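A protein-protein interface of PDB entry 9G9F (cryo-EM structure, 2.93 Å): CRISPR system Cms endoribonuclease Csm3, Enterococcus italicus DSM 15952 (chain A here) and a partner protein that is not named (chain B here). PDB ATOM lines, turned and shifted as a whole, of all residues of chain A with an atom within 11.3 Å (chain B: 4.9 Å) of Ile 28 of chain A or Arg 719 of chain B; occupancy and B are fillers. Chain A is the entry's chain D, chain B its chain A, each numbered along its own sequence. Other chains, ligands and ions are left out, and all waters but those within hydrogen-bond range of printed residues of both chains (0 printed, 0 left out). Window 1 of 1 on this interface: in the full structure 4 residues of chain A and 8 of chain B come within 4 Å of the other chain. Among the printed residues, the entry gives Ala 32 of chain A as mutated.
N of Ile 28 of chain A is in hydrogen-bond range of OH of Tyr 768 of chain B (3.4 Å).
The guanidinium group (NH2) of Arg 719 of chain B lies close to the side-chain sulfur (SD) of Met 27 of chain A (3.7 Å).
SD of Met 27 of chain A lies close to OE2 of Glu 764 of chain B (3.1 Å).
The side-chain hydroxyl of Tyr 768 of chain B sits at hydrogen-bond distance from the backbone carbonyl oxygen of Ser 26 of chain A, at 3.1 Å.
The guanidinium group (NH1) of Arg 719 of chain B is in hydrogen-bond range of the backbone carbonyl oxygen (O) of Ile 28 of chain A, 3.4 Å away.
The backbone carbonyl oxygen (O) of Ile 31 of chain A is in hydrogen-bond range of the side-chain hydroxyl (OG) of Ser 26 of chain A.
The guanidinium group (NH1) of Arg 719 of chain B lies within salt-bridge range of the side-chain carboxylate (OE2) of Glu 764 of chain B, 3.8 Å away.
The backbone NH (N) of Ile 540 of chain B is in hydrogen-bond range of the backbone carbonyl oxygen (O) of Tyr 768 of chain B (2.8 Å).
CA of Met 27 of chain A touches OH of Tyr 768 of chain B, at 3.7 Å.
Ile 28 of chain A touches Tyr 712 of chain B (CG1 to OH, 3.4 Å).
O of Ile 28 of chain A touches CD2 of Leu 715 of chain B (3.8 Å).
CG1 of Ile 28 of chain A touches CG1 of Val 767 of chain B (3.5 Å).
CD1 of Ile 28 of chain A touches NH1 of Arg 771 of chain B, 3.3 Å away.
Arg 719 of chain B touches Ala 30 of chain A.
Printed residues of chain B within 4 Å of Ser 26 of chain A: Tyr 768.
Printed residues of chain B within 4 Å of Ala 30 of chain A: Arg 719 (3.7 Å).
Of the printed residues of chain A, Tyr 712 of chain B touches Ile 28.
No residue of chain A comes within 4 Å of Glu 716 of chain B.
No residue of chain A comes within 4 Å of Leu 718 of chain B.
Of the printed residues of chain A, Arg 719 of chain B touches Met 27, Ile 28 and Ala 30.
Ile 760 of chain B touches none of the printed residues of chain A.
Of the printed residues of chain A, Glu 764 of chain B touches Met 27.
Of the printed residues of chain A, Arg 771 of chain B touches Ile 28 (3.3 Å).
The nearest residue of chain A that does not touch Arg 719 of chain B is Gly 29 of chain A (4.5 Å).
The nearest printed residue of chain A that does not touch Arg 771 of chain B is Gly 29 of chain A (7.0 Å).
Of the 14 printed residues of chain B, 7 touch a printed residue of chain A.
Printed residues of chain B that touch a printed residue of chain A: Tyr 712, Leu 715, Arg 719, Glu 764, Val 767, Tyr 768 and Arg 771.
Of the 15 printed residues of chain A, 4 touch a printed residue of chain B.
Among the printed residues, 11 pairs touch across the chains.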
ATOM      1  N   SER A  26     -26.109 -24.874 -15.152  1.00  0.00           N
ATOM      2  CA  SER A  26     -25.973 -26.323 -15.063  1.00  0.00           C
ATOM      3  C   SER A  26     -26.734 -26.883 -13.862  1.00  0.00           C
ATOM      4  O   SER A  26     -27.725 -26.304 -13.417  1.00  0.00           O
ATOM      5  CB  SER A  26     -24.495 -26.716 -14.987  1.00  0.00           C
ATOM      6  OG  SER A  26     -23.788 -25.879 -14.091  1.00  0.00           O
ATOM      7  N   MET A  27     -26.261 -28.014 -13.344  1.00  0.00           N
ATOM      8  CA  MET A  27     -26.947 -28.685 -12.250  1.00  0.00           C
ATOM      9  C   MET A  27     -26.813 -27.921 -10.941  1.00  0.00           C
ATOM     10  O   MET A  27     -25.878 -27.145 -10.734  1.00  0.00           O
ATOM     11  CB  MET A  27     -26.412 -30.104 -12.072  1.00  0.00           C
ATOM     12  CG  MET A  27     -26.730 -31.029 -13.220  1.00  0.00           C
ATOM     13  SD  MET A  27     -26.132 -32.690 -12.866  1.00  0.00           S
ATOM     14  CE  MET A  27     -24.386 -32.476 -13.147  1.00  0.00           C
ATOM     15  N   ILE A  28     -27.775 -28.159 -10.050  1.00  0.00           N
ATOM     16  CA  ILE A  28     -27.767 -27.526  -8.742  1.00  0.00           C
ATOM     17  C   ILE A  28     -26.606 -28.071  -7.920  1.00  0.00           C
ATOM     18  O   ILE A  28     -26.186 -29.226  -8.078  1.00  0.00           O
ATOM     19  CB  ILE A  28     -29.116 -27.739  -8.032  1.00  0.00           C
ATOM     20  CG1 ILE A  28     -29.338 -26.663  -6.976  1.00  0.00           C
ATOM     21  CG2 ILE A  28     -29.201 -29.121  -7.413  1.00  0.00           C
ATOM     22  CD1 ILE A  28     -29.701 -25.327  -7.554  1.00  0.00           C
ATOM     23  N   GLY A  29     -26.062 -27.225  -7.051  1.00  0.00           N
ATOM     24  CA  GLY A  29     -24.912 -27.615  -6.254  1.00  0.00           C
ATOM     25  C   GLY A  29     -23.689 -27.968  -7.068  1.00  0.00           C
ATOM     26  O   GLY A  29     -22.906 -28.832  -6.660  1.00  0.00           O
ATOM     27  N   ALA A  30     -23.500 -27.323  -8.214  1.00  0.00           N
ATOM     28  CA  ALA A  30     -22.349 -27.561  -9.069  1.00  0.00           C
ATOM     29  C   ALA A  30     -21.721 -26.223  -9.428  1.00  0.00           C
ATOM     30  O   ALA A  30     -22.181 -25.162  -8.996  1.00  0.00           O
ATOM     31  CB  ALA A  30     -22.742 -28.341 -10.328  1.00  0.00           C
ATOM     32  N   ILE A  31     -20.660 -26.275 -10.232  1.00  0.00           N
ATOM     33  CA  ILE A  31     -19.939 -25.074 -10.635  1.00  0.00           C
ATOM     34  C   ILE A  31     -20.881 -24.168 -11.410  1.00  0.00           C
ATOM     35  O   ILE A  31     -21.313 -24.503 -12.518  1.00  0.00           O
ATOM     36  CB  ILE A  31     -18.697 -25.416 -11.476  1.00  0.00           C
ATOM     37  CG1 ILE A  31     -17.654 -26.135 -10.621  1.00  0.00           C
ATOM     38  CG2 ILE A  31     -18.115 -24.159 -12.078  1.00  0.00           C
ATOM     39  CD1 ILE A  31     -16.404 -26.508 -11.383  1.00  0.00           C
ATOM     40  N   ALA A  32     -21.208 -23.014 -10.827  1.00  0.00           N
ATOM     41  CA  ALA A  32     -22.156 -22.109 -11.461  1.00  0.00           C
ATOM     42  C   ALA A  32     -21.575 -21.466 -12.712  1.00  0.00           C
ATOM     43  O   ALA A  32     -22.306 -21.237 -13.684  1.00  0.00           O
ATOM     44  CB  ALA A  32     -22.599 -21.038 -10.467  1.00  0.00           C
ATOM     45  N   SER A  33     -20.278 -21.168 -12.713  1.00  0.00           N
ATOM     46  CA  SER A  33     -19.621 -20.485 -13.826  1.00  0.00           C
ATOM     47  C   SER A  33     -18.372 -21.259 -14.223  1.00  0.00           C
ATOM     48  O   SER A  33     -17.257 -20.911 -13.819  1.00  0.00           O
ATOM     49  CB  SER A  33     -19.280 -19.042 -13.455  1.00  0.00           C
ATOM     50  OG  SER A  33     -20.425 -18.354 -12.984  1.00  0.00           O
ATOM     51  N   PRO A  34     -18.524 -22.322 -15.007  1.00  0.00           N
ATOM     52  CA  PRO A  34     -17.345 -23.058 -15.475  1.00  0.00           C
ATOM     53  C   PRO A  34     -16.537 -22.242 -16.470  1.00  0.00           C
ATOM     54  O   PRO A  34     -17.085 -21.476 -17.264  1.00  0.00           O
ATOM     55  CB  PRO A  34     -17.946 -24.303 -16.133  1.00  0.00           C
ATOM     56  CG  PRO A  34     -19.305 -23.874 -16.557  1.00  0.00           C
ATOM     57  CD  PRO A  34     -19.777 -22.891 -15.526  1.00  0.00           C
ATOM     58  N   THR A 121     -12.294 -25.298  -7.603  1.00  0.00           N
ATOM     59  CA  THR A 121     -13.613 -24.711  -7.388  1.00  0.00           C
ATOM     60  C   THR A 121     -13.545 -23.835  -6.140  1.00  0.00           C
ATOM     61  O   THR A 121     -13.688 -24.320  -5.018  1.00  0.00           O
ATOM     62  CB  THR A 121     -14.673 -25.792  -7.254  1.00  0.00           C
ATOM     63  OG1 THR A 121     -14.738 -26.545  -8.470  1.00  0.00           O
ATOM     64  CG2 THR A 121     -16.028 -25.178  -6.982  1.00  0.00           C
ATOM     65  N   PHE A 123     -15.008 -21.551  -3.474  1.00  0.00           N
ATOM     66  CA  PHE A 123     -16.284 -21.220  -2.870  1.00  0.00           C
ATOM     67  C   PHE A 123     -16.228 -19.783  -2.380  1.00  0.00           C
ATOM     68  O   PHE A 123     -15.306 -19.409  -1.652  1.00  0.00           O
ATOM     69  CB  PHE A 123     -16.604 -22.166  -1.715  1.00  0.00           C
ATOM     70  CG  PHE A 123     -17.122 -23.496  -2.157  1.00  0.00           C
ATOM     71  CD1 PHE A 123     -16.280 -24.418  -2.745  1.00  0.00           C
ATOM     72  CD2 PHE A 123     -18.453 -23.821  -1.993  1.00  0.00           C
ATOM     73  CE1 PHE A 123     -16.751 -25.638  -3.156  1.00  0.00           C
ATOM     74  CE2 PHE A 123     -18.930 -25.042  -2.401  1.00  0.00           C
ATOM     75  CZ  PHE A 123     -18.078 -25.952  -2.983  1.00  0.00           C
ATOM     76  N   ASN A 135     -24.474 -15.502  -0.222  1.00  0.00           N
ATOM     77  CA  ASN A 135     -24.897 -16.199  -1.437  1.00  0.00           C
ATOM     78  C   ASN A 135     -23.752 -17.046  -1.971  1.00  0.00           C
ATOM     79  O   ASN A 135     -22.795 -16.489  -2.547  1.00  0.00           O
ATOM     80  CB  ASN A 135     -25.369 -15.198  -2.486  1.00  0.00           C
ATOM     81  CG  ASN A 135     -26.415 -15.774  -3.411  1.00  0.00           C
ATOM     82  OD1 ASN A 135     -26.168 -15.965  -4.599  1.00  0.00           O
ATOM     83  ND2 ASN A 135     -27.594 -16.048  -2.872  1.00  0.00           N
ATOM     84  N   PRO A 136     -23.807 -18.369  -1.833  1.00  0.00           N
ATOM     85  CA  PRO A 136     -22.680 -19.202  -2.258  1.00  0.00           C
ATOM     86  C   PRO A 136     -22.470 -19.121  -3.758  1.00  0.00           C
ATOM     87  O   PRO A 136     -23.398 -18.873  -4.529  1.00  0.00           O
ATOM     88  CB  PRO A 136     -23.094 -20.615  -1.835  1.00  0.00           C
ATOM     89  CG  PRO A 136     -24.246 -20.439  -0.928  1.00  0.00           C
ATOM     90  CD  PRO A 136     -24.924 -19.186  -1.347  1.00  0.00           C
ATOM     91  N   ARG A 137     -21.229 -19.337  -4.167  1.00  0.00           N
ATOM     92  CA  ARG A 137     -20.847 -19.153  -5.558  1.00  0.00           C
ATOM     93  C   ARG A 137     -19.615 -20.009  -5.802  1.00  0.00           C
ATOM     94  O   ARG A 137     -18.565 -19.761  -5.208  1.00  0.00           O
ATOM     95  CB  ARG A 137     -20.582 -17.678  -5.842  1.00  0.00           C
ATOM     96  CG  ARG A 137     -19.746 -17.407  -7.055  1.00  0.00           C
ATOM     97  CD  ARG A 137     -19.683 -15.924  -7.366  1.00  0.00           C
ATOM     98  NE  ARG A 137     -18.743 -15.201  -6.519  1.00  0.00           N
ATOM     99  CZ  ARG A 137     -19.080 -14.547  -5.418  1.00  0.00           C
ATOM    100  NH1 ARG A 137     -20.320 -14.553  -4.962  1.00  0.00           N
ATOM    101  NH2 ARG A 137     -18.149 -13.866  -4.757  1.00  0.00           N
ATOM    102  N   GLN A 138     -19.747 -21.030  -6.636  1.00  0.00           N
ATOM    103  CA  GLN A 138     -18.656 -21.959  -6.903  1.00  0.00           C
ATOM    104  C   GLN A 138     -18.032 -21.581  -8.237  1.00  0.00           C
ATOM    105  O   GLN A 138     -18.493 -22.009  -9.296  1.00  0.00           O
ATOM    106  CB  GLN A 138     -19.156 -23.397  -6.896  1.00  0.00           C
ATOM    107  CG  GLN A 138     -19.885 -23.767  -5.623  1.00  0.00           C
ATOM    108  CD  GLN A 138     -20.274 -25.223  -5.580  1.00  0.00           C
ATOM    109  OE1 GLN A 138     -19.730 -26.043  -6.317  1.00  0.00           O
ATOM    110  NE2 GLN A 138     -21.224 -25.554  -4.718  1.00  0.00           N
ATOM    111  N   ILE B 540     -37.778 -22.735  -8.036  1.00  0.00           N
ATOM    112  CA  ILE B 540     -36.735 -21.957  -8.708  1.00  0.00           C
ATOM    113  C   ILE B 540     -37.331 -21.282  -9.940  1.00  0.00           C
ATOM    114  O   ILE B 540     -38.091 -21.923 -10.688  1.00  0.00           O
ATOM    115  CB  ILE B 540     -35.548 -22.860  -9.068  1.00  0.00           C
ATOM    116  CG1 ILE B 540     -34.357 -22.041  -9.550  1.00  0.00           C
ATOM    117  CG2 ILE B 540     -35.929 -23.910 -10.093  1.00  0.00           C
ATOM    118  CD1 ILE B 540     -33.148 -22.886  -9.859  1.00  0.00           C
ATOM    119  N   TYR B 712     -28.614 -31.378   0.224  1.00  0.00           N
ATOM    120  CA  TYR B 712     -27.403 -30.996  -0.494  1.00  0.00           C
ATOM    121  C   TYR B 712     -26.229 -31.879  -0.096  1.00  0.00           C
ATOM    122  O   TYR B 712     -25.388 -32.217  -0.934  1.00  0.00           O
ATOM    123  CB  TYR B 712     -27.083 -29.526  -0.242  1.00  0.00           C
ATOM    124  CG  TYR B 712     -27.799 -28.574  -1.171  1.00  0.00           C
ATOM    125  CD1 TYR B 712     -27.370 -28.394  -2.475  1.00  0.00           C
ATOM    126  CD2 TYR B 712     -28.897 -27.845  -0.736  1.00  0.00           C
ATOM    127  CE1 TYR B 712     -28.018 -27.521  -3.321  1.00  0.00           C
ATOM    128  CE2 TYR B 712     -29.549 -26.972  -1.574  1.00  0.00           C
ATOM    129  CZ  TYR B 712     -29.107 -26.814  -2.865  1.00  0.00           C
ATOM    130  OH  TYR B 712     -29.755 -25.938  -3.703  1.00  0.00           O
ATOM    131  N   LEU B 715     -26.720 -35.073  -1.920  1.00  0.00           N
ATOM    132  CA  LEU B 715     -26.377 -34.876  -3.323  1.00  0.00           C
ATOM    133  C   LEU B 715     -24.867 -34.847  -3.519  1.00  0.00           C
ATOM    134  O   LEU B 715     -24.347 -35.437  -4.468  1.00  0.00           O
ATOM    135  CB  LEU B 715     -27.016 -33.587  -3.841  1.00  0.00           C
ATOM    136  CG  LEU B 715     -26.680 -33.202  -5.282  1.00  0.00           C
ATOM    137  CD1 LEU B 715     -27.136 -34.286  -6.238  1.00  0.00           C
ATOM    138  CD2 LEU B 715     -27.306 -31.871  -5.645  1.00  0.00           C
ATOM    139  N   GLU B 716     -24.147 -34.167  -2.629  1.00  0.00           N
ATOM    140  CA  GLU B 716     -22.694 -34.130  -2.734  1.00  0.00           C
ATOM    141  C   GLU B 716     -22.098 -35.518  -2.574  1.00  0.00           C
ATOM    142  O   GLU B 716     -21.141 -35.875  -3.269  1.00  0.00           O
ATOM    143  CB  GLU B 716     -22.115 -33.172  -1.695  1.00  0.00           C
ATOM    144  CG  GLU B 716     -20.578 -33.001  -1.666  1.00  0.00           C
ATOM    145  CD  GLU B 716     -19.829 -32.985  -3.014  1.00  0.00           C
ATOM    146  OE1 GLU B 716     -18.594 -32.821  -2.956  1.00  0.00           O
ATOM    147  OE2 GLU B 716     -20.421 -33.059  -4.116  1.00  0.00           O
ATOM    148  N   LEU B 717     -22.645 -36.313  -1.653  1.00  0.00           N
ATOM    149  CA  LEU B 717     -22.177 -37.687  -1.506  1.00  0.00           C
ATOM    150  C   LEU B 717     -22.445 -38.500  -2.768  1.00  0.00           C
ATOM    151  O   LEU B 717     -21.586 -39.270  -3.213  1.00  0.00           O
ATOM    152  CB  LEU B 717     -22.846 -38.343  -0.301  1.00  0.00           C
ATOM    153  CG  LEU B 717     -22.465 -37.801   1.074  1.00  0.00           C
ATOM    154  CD1 LEU B 717     -23.456 -38.269   2.115  1.00  0.00           C
ATOM    155  CD2 LEU B 717     -21.062 -38.226   1.438  1.00  0.00           C
ATOM    156  N   LEU B 718     -23.629 -38.334  -3.364  1.00  0.00           N
ATOM    157  CA  LEU B 718     -24.022 -39.177  -4.490  1.00  0.00           C
ATOM    158  C   LEU B 718     -23.272 -38.808  -5.766  1.00  0.00           C
ATOM    159  O   LEU B 718     -22.914 -39.691  -6.555  1.00  0.00           O
ATOM    160  CB  LEU B 718     -25.531 -39.086  -4.706  1.00  0.00           C
ATOM    161  CG  LEU B 718     -26.379 -39.757  -3.628  1.00  0.00           C
ATOM    162  CD1 LEU B 718     -27.801 -39.238  -3.657  1.00  0.00           C
ATOM    163  CD2 LEU B 718     -26.360 -41.258  -3.807  1.00  0.00           C
ATOM    164  N   ARG B 719     -23.031 -37.516  -5.993  1.00  0.00           N
ATOM    165  CA  ARG B 719     -22.340 -37.101  -7.210  1.00  0.00           C
ATOM    166  C   ARG B 719     -20.912 -37.629  -7.245  1.00  0.00           C
ATOM    167  O   ARG B 719     -20.390 -37.956  -8.317  1.00  0.00           O
ATOM    168  CB  ARG B 719     -22.349 -35.578  -7.334  1.00  0.00           C
ATOM    169  CG  ARG B 719     -23.735 -34.966  -7.411  1.00  0.00           C
ATOM    170  CD  ARG B 719     -24.291 -35.010  -8.817  1.00  0.00           C
ATOM    171  NE  ARG B 719     -23.642 -34.040  -9.689  1.00  0.00           N
ATOM    172  CZ  ARG B 719     -23.923 -32.745  -9.707  1.00  0.00           C
ATOM    173  NH1 ARG B 719     -24.833 -32.223  -8.900  1.00  0.00           N
ATOM    174  NH2 ARG B 719     -23.276 -31.953 -10.556  1.00  0.00           N
ATOM    175  N   ASN B 720     -20.261 -37.709  -6.087  1.00  0.00           N
ATOM    176  CA  ASN B 720     -18.899 -38.221  -6.034  1.00  0.00           C
ATOM    177  C   ASN B 720     -18.859 -39.679  -6.471  1.00  0.00           C
ATOM    178  O   ASN B 720     -19.666 -40.500  -6.031  1.00  0.00           O
ATOM    179  CB  ASN B 720     -18.329 -38.078  -4.624  1.00  0.00           C
ATOM    180  CG  ASN B 720     -18.252 -36.637  -4.170  1.00  0.00           C
ATOM    181  OD1 ASN B 720     -18.410 -36.339  -2.987  1.00  0.00           O
ATOM    182  ND2 ASN B 720     -18.014 -35.732  -5.110  1.00  0.00           N
ATOM    183  N   GLU B 721     -17.907 -39.994  -7.347  1.00  0.00           N
ATOM    184  CA  GLU B 721     -17.770 -41.334  -7.900  1.00  0.00           C
ATOM    185  C   GLU B 721     -16.935 -42.263  -7.029  1.00  0.00           C
ATOM    186  O   GLU B 721     -16.927 -43.474  -7.278  1.00  0.00           O
ATOM    187  CB  GLU B 721     -17.153 -41.260  -9.302  1.00  0.00           C
ATOM    188  CG  GLU B 721     -17.453 -42.461 -10.182  1.00  0.00           C
ATOM    189  CD  GLU B 721     -16.950 -42.285 -11.598  1.00  0.00           C
ATOM    190  OE1 GLU B 721     -16.697 -41.129 -11.999  1.00  0.00           O
ATOM    191  OE2 GLU B 721     -16.806 -43.301 -12.310  1.00  0.00           O
ATOM    192  N   ILE B 760     -30.182 -39.133  -7.798  1.00  0.00           N
ATOM    193  CA  ILE B 760     -29.563 -37.838  -8.068  1.00  0.00           C
ATOM    194  C   ILE B 760     -30.554 -36.919  -8.768  1.00  0.00           C
ATOM    195  O   ILE B 760     -30.723 -35.752  -8.393  1.00  0.00           O
ATOM    196  CB  ILE B 760     -28.283 -38.019  -8.905  1.00  0.00           C
ATOM    197  CG1 ILE B 760     -27.172 -38.647  -8.068  1.00  0.00           C
ATOM    198  CG2 ILE B 760     -27.823 -36.693  -9.479  1.00  0.00           C
ATOM    199  CD1 ILE B 760     -25.922 -38.936  -8.860  1.00  0.00           C
ATOM    200  N   GLU B 764     -32.170 -33.437  -7.343  1.00  0.00           N
ATOM    201  CA  GLU B 764     -32.053 -32.181  -8.077  1.00  0.00           C
ATOM    202  C   GLU B 764     -33.423 -31.583  -8.358  1.00  0.00           C
ATOM    203  O   GLU B 764     -33.622 -30.371  -8.216  1.00  0.00           O
ATOM    204  CB  GLU B 764     -31.294 -32.406  -9.382  1.00  0.00           C
ATOM    205  CG  GLU B 764     -29.842 -32.787  -9.204  1.00  0.00           C
ATOM    206  CD  GLU B 764     -29.125 -32.934 -10.529  1.00  0.00           C
ATOM    207  OE1 GLU B 764     -29.698 -32.521 -11.557  1.00  0.00           O
ATOM    208  OE2 GLU B 764     -27.994 -33.463 -10.549  1.00  0.00           O
ATOM    209  N   VAL B 767     -34.830 -30.140  -5.123  1.00  0.00           N
ATOM    210  CA  VAL B 767     -34.146 -28.903  -4.764  1.00  0.00           C
ATOM    211  C   VAL B 767     -34.620 -27.757  -5.647  1.00  0.00           C
ATOM    212  O   VAL B 767     -34.877 -26.649  -5.165  1.00  0.00           O
ATOM    213  CB  VAL B 767     -32.623 -29.094  -4.849  1.00  0.00           C
ATOM    214  CG1 VAL B 767     -31.942 -27.757  -4.889  1.00  0.00           C
ATOM    215  CG2 VAL B 767     -32.130 -29.906  -3.665  1.00  0.00           C
ATOM    216  N   TYR B 768     -34.755 -28.010  -6.951  1.00  0.00           N
ATOM    217  CA  TYR B 768     -35.279 -26.991  -7.853  1.00  0.00           C
ATOM    218  C   TYR B 768     -36.680 -26.567  -7.442  1.00  0.00           C
ATOM    219  O   TYR B 768     -36.994 -25.374  -7.413  1.00  0.00           O
ATOM    220  CB  TYR B 768     -35.293 -27.523  -9.283  1.00  0.00           C
ATOM    221  CG  TYR B 768     -33.970 -27.444 -10.001  1.00  0.00           C
ATOM    222  CD1 TYR B 768     -33.046 -26.464  -9.689  1.00  0.00           C
ATOM    223  CD2 TYR B 768     -33.651 -28.349 -10.996  1.00  0.00           C
ATOM    224  CE1 TYR B 768     -31.840 -26.390 -10.348  1.00  0.00           C
ATOM    225  CE2 TYR B 768     -32.449 -28.285 -11.658  1.00  0.00           C
ATOM    226  CZ  TYR B 768     -31.547 -27.304 -11.332  1.00  0.00           C
ATOM    227  OH  TYR B 768     -30.346 -27.239 -11.997  1.00  0.00           O
ATOM    228  N   ARG B 771     -36.577 -24.409  -4.135  1.00  0.00           N
ATOM    229  CA  ARG B 771     -35.749 -23.211  -4.088  1.00  0.00           C
ATOM    230  C   ARG B 771     -36.600 -21.973  -3.824  1.00  0.00           C
ATOM    231  O   ARG B 771     -37.809 -21.952  -4.068  1.00  0.00           O
ATOM    232  CB  ARG B 771     -34.984 -23.039  -5.399  1.00  0.00           C
ATOM    233  CG  ARG B 771     -33.643 -23.746  -5.442  1.00  0.00           C
ATOM    234  CD  ARG B 771     -32.530 -22.859  -4.941  1.00  0.00           C
ATOM    235  NE  ARG B 771     -32.482 -21.597  -5.667  1.00  0.00           N
ATOM    236  CZ  ARG B 771     -31.768 -21.393  -6.764  1.00  0.00           C
ATOM    237  NH1 ARG B 771     -31.039 -22.356  -7.302  1.00  0.00           N
ATOM    238  NH2 ARG B 771     -31.784 -20.192  -7.334  1.00  0.00           N
